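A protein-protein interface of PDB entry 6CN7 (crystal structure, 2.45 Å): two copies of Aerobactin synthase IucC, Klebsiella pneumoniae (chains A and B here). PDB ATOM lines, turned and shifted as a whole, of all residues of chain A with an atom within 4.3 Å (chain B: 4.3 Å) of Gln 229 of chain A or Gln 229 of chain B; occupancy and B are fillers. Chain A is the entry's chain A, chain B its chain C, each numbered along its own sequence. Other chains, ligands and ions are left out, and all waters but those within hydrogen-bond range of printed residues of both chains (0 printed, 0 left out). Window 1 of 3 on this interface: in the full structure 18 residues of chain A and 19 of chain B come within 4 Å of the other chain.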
ATOM      1  N   TRP A 225     -23.463   9.724  15.146  1.00  0.00           N
ATOM      2  CA  TRP A 225     -22.782   9.201  13.965  1.00  0.00           C
ATOM      3  C   TRP A 225     -21.286   9.075  14.214  1.00  0.00           C
ATOM      4  O   TRP A 225     -20.672   8.063  13.858  1.00  0.00           O
ATOM      5  CB  TRP A 225     -23.044  10.097  12.754  1.00  0.00           C
ATOM      6  CG  TRP A 225     -22.519   9.510  11.475  1.00  0.00           C
ATOM      7  CD1 TRP A 225     -23.213   8.754  10.573  1.00  0.00           C
ATOM      8  CD2 TRP A 225     -21.186   9.620  10.963  1.00  0.00           C
ATOM      9  NE1 TRP A 225     -22.398   8.390   9.533  1.00  0.00           N
ATOM     10  CE2 TRP A 225     -21.146   8.907   9.747  1.00  0.00           C
ATOM     11  CE3 TRP A 225     -20.021  10.249  11.414  1.00  0.00           C
ATOM     12  CZ2 TRP A 225     -19.986   8.808   8.975  1.00  0.00           C
ATOM     13  CZ3 TRP A 225     -18.875  10.151  10.647  1.00  0.00           C
ATOM     14  CH2 TRP A 225     -18.867   9.437   9.441  1.00  0.00           C
ATOM     15  N   GLN A 226     -20.684  10.095  14.832  1.00  0.00           N
ATOM     16  CA  GLN A 226     -19.264  10.034  15.160  1.00  0.00           C
ATOM     17  C   GLN A 226     -18.963   8.850  16.070  1.00  0.00           C
ATOM     18  O   GLN A 226     -17.978   8.131  15.860  1.00  0.00           O
ATOM     19  CB  GLN A 226     -18.831  11.345  15.816  1.00  0.00           C
ATOM     20  CG  GLN A 226     -17.332  11.470  16.068  1.00  0.00           C
ATOM     21  CD  GLN A 226     -16.542  11.759  14.809  1.00  0.00           C
ATOM     22  OE1 GLN A 226     -17.075  11.716  13.701  1.00  0.00           O
ATOM     23  NE2 GLN A 226     -15.259  12.063  14.974  1.00  0.00           N
ATOM     24  N   TRP A 227     -19.796   8.630  17.091  1.00  0.00           N
ATOM     25  CA  TRP A 227     -19.597   7.478  17.966  1.00  0.00           C
ATOM     26  C   TRP A 227     -19.806   6.174  17.211  1.00  0.00           C
ATOM     27  O   TRP A 227     -19.019   5.229  17.352  1.00  0.00           O
ATOM     28  CB  TRP A 227     -20.547   7.541  19.159  1.00  0.00           C
ATOM     29  CG  TRP A 227     -20.609   6.245  19.906  1.00  0.00           C
ATOM     30  CD1 TRP A 227     -21.629   5.337  19.896  1.00  0.00           C
ATOM     31  CD2 TRP A 227     -19.597   5.700  20.757  1.00  0.00           C
ATOM     32  NE1 TRP A 227     -21.317   4.263  20.695  1.00  0.00           N
ATOM     33  CE2 TRP A 227     -20.074   4.463  21.236  1.00  0.00           C
ATOM     34  CE3 TRP A 227     -18.335   6.140  21.164  1.00  0.00           C
ATOM     35  CZ2 TRP A 227     -19.333   3.663  22.102  1.00  0.00           C
ATOM     36  CZ3 TRP A 227     -17.600   5.345  22.024  1.00  0.00           C
ATOM     37  CH2 TRP A 227     -18.101   4.121  22.484  1.00  0.00           C
ATOM     38  N   GLN A 228     -20.869   6.109  16.410  1.00  0.00           N
ATOM     39  CA  GLN A 228     -21.228   4.877  15.720  1.00  0.00           C
ATOM     40  C   GLN A 228     -20.134   4.447  14.748  1.00  0.00           C
ATOM     41  O   GLN A 228     -19.706   3.287  14.748  1.00  0.00           O
ATOM     42  CB  GLN A 228     -22.555   5.090  14.994  1.00  0.00           C
ATOM     43  CG  GLN A 228     -23.163   3.867  14.341  1.00  0.00           C
ATOM     44  CD  GLN A 228     -24.449   4.205  13.614  1.00  0.00           C
ATOM     45  OE1 GLN A 228     -24.578   3.965  12.414  1.00  0.00           O
ATOM     46  NE2 GLN A 228     -25.406   4.781  14.336  1.00  0.00           N
ATOM     47  N   GLN A 229     -19.655   5.377  13.923  1.00  0.00           N
ATOM     48  CA  GLN A 229     -18.777   5.038  12.810  1.00  0.00           C
ATOM     49  C   GLN A 229     -17.294   5.182  13.116  1.00  0.00           C
ATOM     50  O   GLN A 229     -16.485   4.465  12.517  1.00  0.00           O
ATOM     51  CB  GLN A 229     -19.109   5.913  11.596  1.00  0.00           C
ATOM     52  CG  GLN A 229     -20.530   5.751  11.089  1.00  0.00           C
ATOM     53  CD  GLN A 229     -20.862   4.315  10.746  1.00  0.00           C
ATOM     54  OE1 GLN A 229     -20.070   3.615  10.115  1.00  0.00           O
ATOM     55  NE2 GLN A 229     -22.036   3.862  11.166  1.00  0.00           N
ATOM     56  N   LYS A 230     -16.905   6.084  14.015  1.00  0.00           N
ATOM     57  CA  LYS A 230     -15.495   6.423  14.189  1.00  0.00           C
ATOM     58  C   LYS A 230     -14.976   6.084  15.579  1.00  0.00           C
ATOM     59  O   LYS A 230     -14.030   5.300  15.701  1.00  0.00           O
ATOM     60  CB  LYS A 230     -15.286   7.911  13.880  1.00  0.00           C
ATOM     61  CG  LYS A 230     -15.594   8.297  12.436  1.00  0.00           C
ATOM     62  CD  LYS A 230     -14.694   7.564  11.447  1.00  0.00           C
ATOM     63  CE  LYS A 230     -14.916   8.052  10.028  1.00  0.00           C
ATOM     64  NZ  LYS A 230     -14.099   7.312   9.028  1.00  0.00           N
ATOM     65  N   ILE A 231     -15.566   6.642  16.635  1.00  0.00           N
ATOM     66  CA  ILE A 231     -14.949   6.553  17.954  1.00  0.00           C
ATOM     67  C   ILE A 231     -15.097   5.152  18.531  1.00  0.00           C
ATOM     68  O   ILE A 231     -14.147   4.600  19.098  1.00  0.00           O
ATOM     69  CB  ILE A 231     -15.542   7.630  18.877  1.00  0.00           C
ATOM     70  CG1 ILE A 231     -15.183   9.017  18.335  1.00  0.00           C
ATOM     71  CG2 ILE A 231     -15.027   7.470  20.308  1.00  0.00           C
ATOM     72  CD1 ILE A 231     -16.027  10.126  18.879  1.00  0.00           C
ATOM     73  N   TRP B 225     -27.054  -4.305  10.898  1.00  0.00           N
ATOM     74  CA  TRP B 225     -25.686  -3.897  10.582  1.00  0.00           C
ATOM     75  C   TRP B 225     -25.456  -3.891   9.076  1.00  0.00           C
ATOM     76  O   TRP B 225     -24.799  -2.990   8.542  1.00  0.00           O
ATOM     77  CB  TRP B 225     -24.674  -4.817  11.270  1.00  0.00           C
ATOM     78  CG  TRP B 225     -23.251  -4.330  11.152  1.00  0.00           C
ATOM     79  CD1 TRP B 225     -22.572  -3.556  12.050  1.00  0.00           C
ATOM     80  CD2 TRP B 225     -22.342  -4.577  10.070  1.00  0.00           C
ATOM     81  NE1 TRP B 225     -21.300  -3.308  11.596  1.00  0.00           N
ATOM     82  CE2 TRP B 225     -21.133  -3.925  10.384  1.00  0.00           C
ATOM     83  CE3 TRP B 225     -22.432  -5.289   8.868  1.00  0.00           C
ATOM     84  CZ2 TRP B 225     -20.023  -3.961   9.541  1.00  0.00           C
ATOM     85  CZ3 TRP B 225     -21.327  -5.321   8.033  1.00  0.00           C
ATOM     86  CH2 TRP B 225     -20.140  -4.663   8.374  1.00  0.00           C
ATOM     87  N   GLN B 226     -25.995  -4.890   8.374  1.00  0.00           N
ATOM     88  CA  GLN B 226     -25.849  -4.944   6.922  1.00  0.00           C
ATOM     89  C   GLN B 226     -26.518  -3.747   6.256  1.00  0.00           C
ATOM     90  O   GLN B 226     -25.959  -3.152   5.327  1.00  0.00           O
ATOM     91  CB  GLN B 226     -26.432  -6.255   6.396  1.00  0.00           C
ATOM     92  CG  GLN B 226     -26.182  -6.509   4.915  1.00  0.00           C
ATOM     93  CD  GLN B 226     -24.742  -6.873   4.614  1.00  0.00           C
ATOM     94  OE1 GLN B 226     -23.884  -6.863   5.499  1.00  0.00           O
ATOM     95  NE2 GLN B 226     -24.469  -7.209   3.358  1.00  0.00           N
ATOM     96  N   TRP B 227     -27.719  -3.382   6.708  1.00  0.00           N
ATOM     97  CA  TRP B 227     -28.375  -2.190   6.180  1.00  0.00           C
ATOM     98  C   TRP B 227     -27.578  -0.940   6.522  1.00  0.00           C
ATOM     99  O   TRP B 227     -27.262  -0.124   5.649  1.00  0.00           O
ATOM    100  CB  TRP B 227     -29.794  -2.071   6.738  1.00  0.00           C
ATOM    101  CG  TRP B 227     -30.389  -0.722   6.481  1.00  0.00           C
ATOM    102  CD1 TRP B 227     -30.603   0.274   7.392  1.00  0.00           C
ATOM    103  CD2 TRP B 227     -30.826  -0.211   5.219  1.00  0.00           C
ATOM    104  NE1 TRP B 227     -31.153   1.371   6.773  1.00  0.00           N
ATOM    105  CE2 TRP B 227     -31.301   1.098   5.439  1.00  0.00           C
ATOM    106  CE3 TRP B 227     -30.865  -0.734   3.924  1.00  0.00           C
ATOM    107  CZ2 TRP B 227     -31.810   1.887   4.411  1.00  0.00           C
ATOM    108  CZ3 TRP B 227     -31.370   0.050   2.908  1.00  0.00           C
ATOM    109  CH2 TRP B 227     -31.836   1.346   3.156  1.00  0.00           C
ATOM    110  N   GLN B 228     -27.244  -0.787   7.801  1.00  0.00           N
ATOM    111  CA  GLN B 228     -26.595   0.423   8.290  1.00  0.00           C
ATOM    112  C   GLN B 228     -25.298   0.707   7.538  1.00  0.00           C
ATOM    113  O   GLN B 228     -25.079   1.824   7.056  1.00  0.00           O
ATOM    114  CB  GLN B 228     -26.347   0.261   9.788  1.00  0.00           C
ATOM    115  CG  GLN B 228     -25.866   1.486  10.533  1.00  0.00           C
ATOM    116  CD  GLN B 228     -25.621   1.174  12.000  1.00  0.00           C
ATOM    117  OE1 GLN B 228     -24.547   1.447  12.536  1.00  0.00           O
ATOM    118  NE2 GLN B 228     -26.620   0.585  12.652  1.00  0.00           N
ATOM    119  N   GLN B 229     -24.430  -0.298   7.414  1.00  0.00           N
ATOM    120  CA  GLN B 229     -23.072  -0.063   6.940  1.00  0.00           C
ATOM    121  C   GLN B 229     -22.893  -0.280   5.446  1.00  0.00           C
ATOM    122  O   GLN B 229     -22.050   0.385   4.832  1.00  0.00           O
ATOM    123  CB  GLN B 229     -22.091  -0.974   7.685  1.00  0.00           C
ATOM    124  CG  GLN B 229     -22.097  -0.791   9.192  1.00  0.00           C
ATOM    125  CD  GLN B 229     -21.925   0.655   9.605  1.00  0.00           C
ATOM    126  OE1 GLN B 229     -22.741   1.201  10.345  1.00  0.00           O
ATOM    127  NE2 GLN B 229     -20.855   1.285   9.131  1.00  0.00           N
ATOM    128  N   LYS B 230     -23.651  -1.192   4.839  1.00  0.00           N
ATOM    129  CA  LYS B 230     -23.379  -1.633   3.476  1.00  0.00           C
ATOM    130  C   LYS B 230     -24.473  -1.237   2.493  1.00  0.00           C
ATOM    131  O   LYS B 230     -24.207  -0.508   1.535  1.00  0.00           O
ATOM    132  CB  LYS B 230     -23.176  -3.155   3.463  1.00  0.00           C
ATOM    133  CG  LYS B 230     -21.942  -3.621   4.222  1.00  0.00           C
ATOM    134  CD  LYS B 230     -20.669  -3.035   3.623  1.00  0.00           C
ATOM    135  CE  LYS B 230     -19.431  -3.581   4.295  1.00  0.00           C
ATOM    136  NZ  LYS B 230     -18.186  -2.970   3.757  1.00  0.00           N
ATOM    137  N   ILE B 231     -25.704  -1.700   2.704  1.00  0.00           N
ATOM    138  CA  ILE B 231     -26.730  -1.572   1.672  1.00  0.00           C
ATOM    139  C   ILE B 231     -27.174  -0.124   1.522  1.00  0.00           C
ATOM    140  O   ILE B 231     -27.293   0.390   0.404  1.00  0.00           O
ATOM    141  CB  ILE B 231     -27.911  -2.506   1.989  1.00  0.00           C
ATOM    142  CG1 ILE B 231     -27.449  -3.958   1.870  1.00  0.00           C
ATOM    143  CG2 ILE B 231     -29.086  -2.246   1.047  1.00  0.00           C
ATOM    144  CD1 ILE B 231     -28.321  -4.930   2.592  1.00  0.00           C
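OE1 of Gln 229 of chain A is in hydrogen-bond range of NE2 of Gln 229 of chain B (2.6 Å).
The side-chain amide oxygen (OE1) of Gln 228 of chain B lies close to the side-chain amide oxygen (OE1) of Gln 228 of chain A, at 2.5 Å.
The side-chain amide oxygen (OE1) of Gln 228 of chain B sits close to the side-chain amide oxygen (OE1) of Gln 229 of chain B (2.9 Å).
OE1 of Gln 228 of chain A lies within hydrogen-bond range of NE2 of Gln 229 of chain A, 2.8 Å away.
Among the printed residues, pairs that only touch across the chains: Gln 228 of chain A with Gln 229 of chain B (3.9 Å) and Gln 229 of chain A with Gln 228 of chain B (3.7 Å).
Gln 229 of chain A touches two residues of chain B.
Of chain A, only Gln 228 (3.9 Å) and Gln 229 (2.6 Å) come within 4 Å of Gln 229 of chain B.
Printed residues of chain B within 4 Å of Gln 228 of chain A: Gln 228 and Gln 229.
Of the printed residues of chain A, Gln 228 of chain B touches Gln 228 (2.5 Å) and Gln 229 (3.7 Å).
Lys 230 of chain B touches none of the printed residues of chain A.
Trp 227 of chain A touches none of the printed residues of chain B.
The nearest printed residue of chain B that does not touch Gln 228 of chain A is Trp 225 of chain B (7.5 Å).
Of the 7 printed residues of chain B, 2 touch a printed residue of chain A.
Gln 228 of chain B touches its own counterpart, Gln 228 of chain A.
Gln 228 of chain A touches Gln 229 of chain B, and with the chains exchanged Gln 229 of chain A touches Gln 228 of chain B.
Gln 229 of chain B touches its own counterpart, Gln 229 of chain A.
Positions printed for both chains: 225, 226, 227, 228, 229, 230 and 231.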
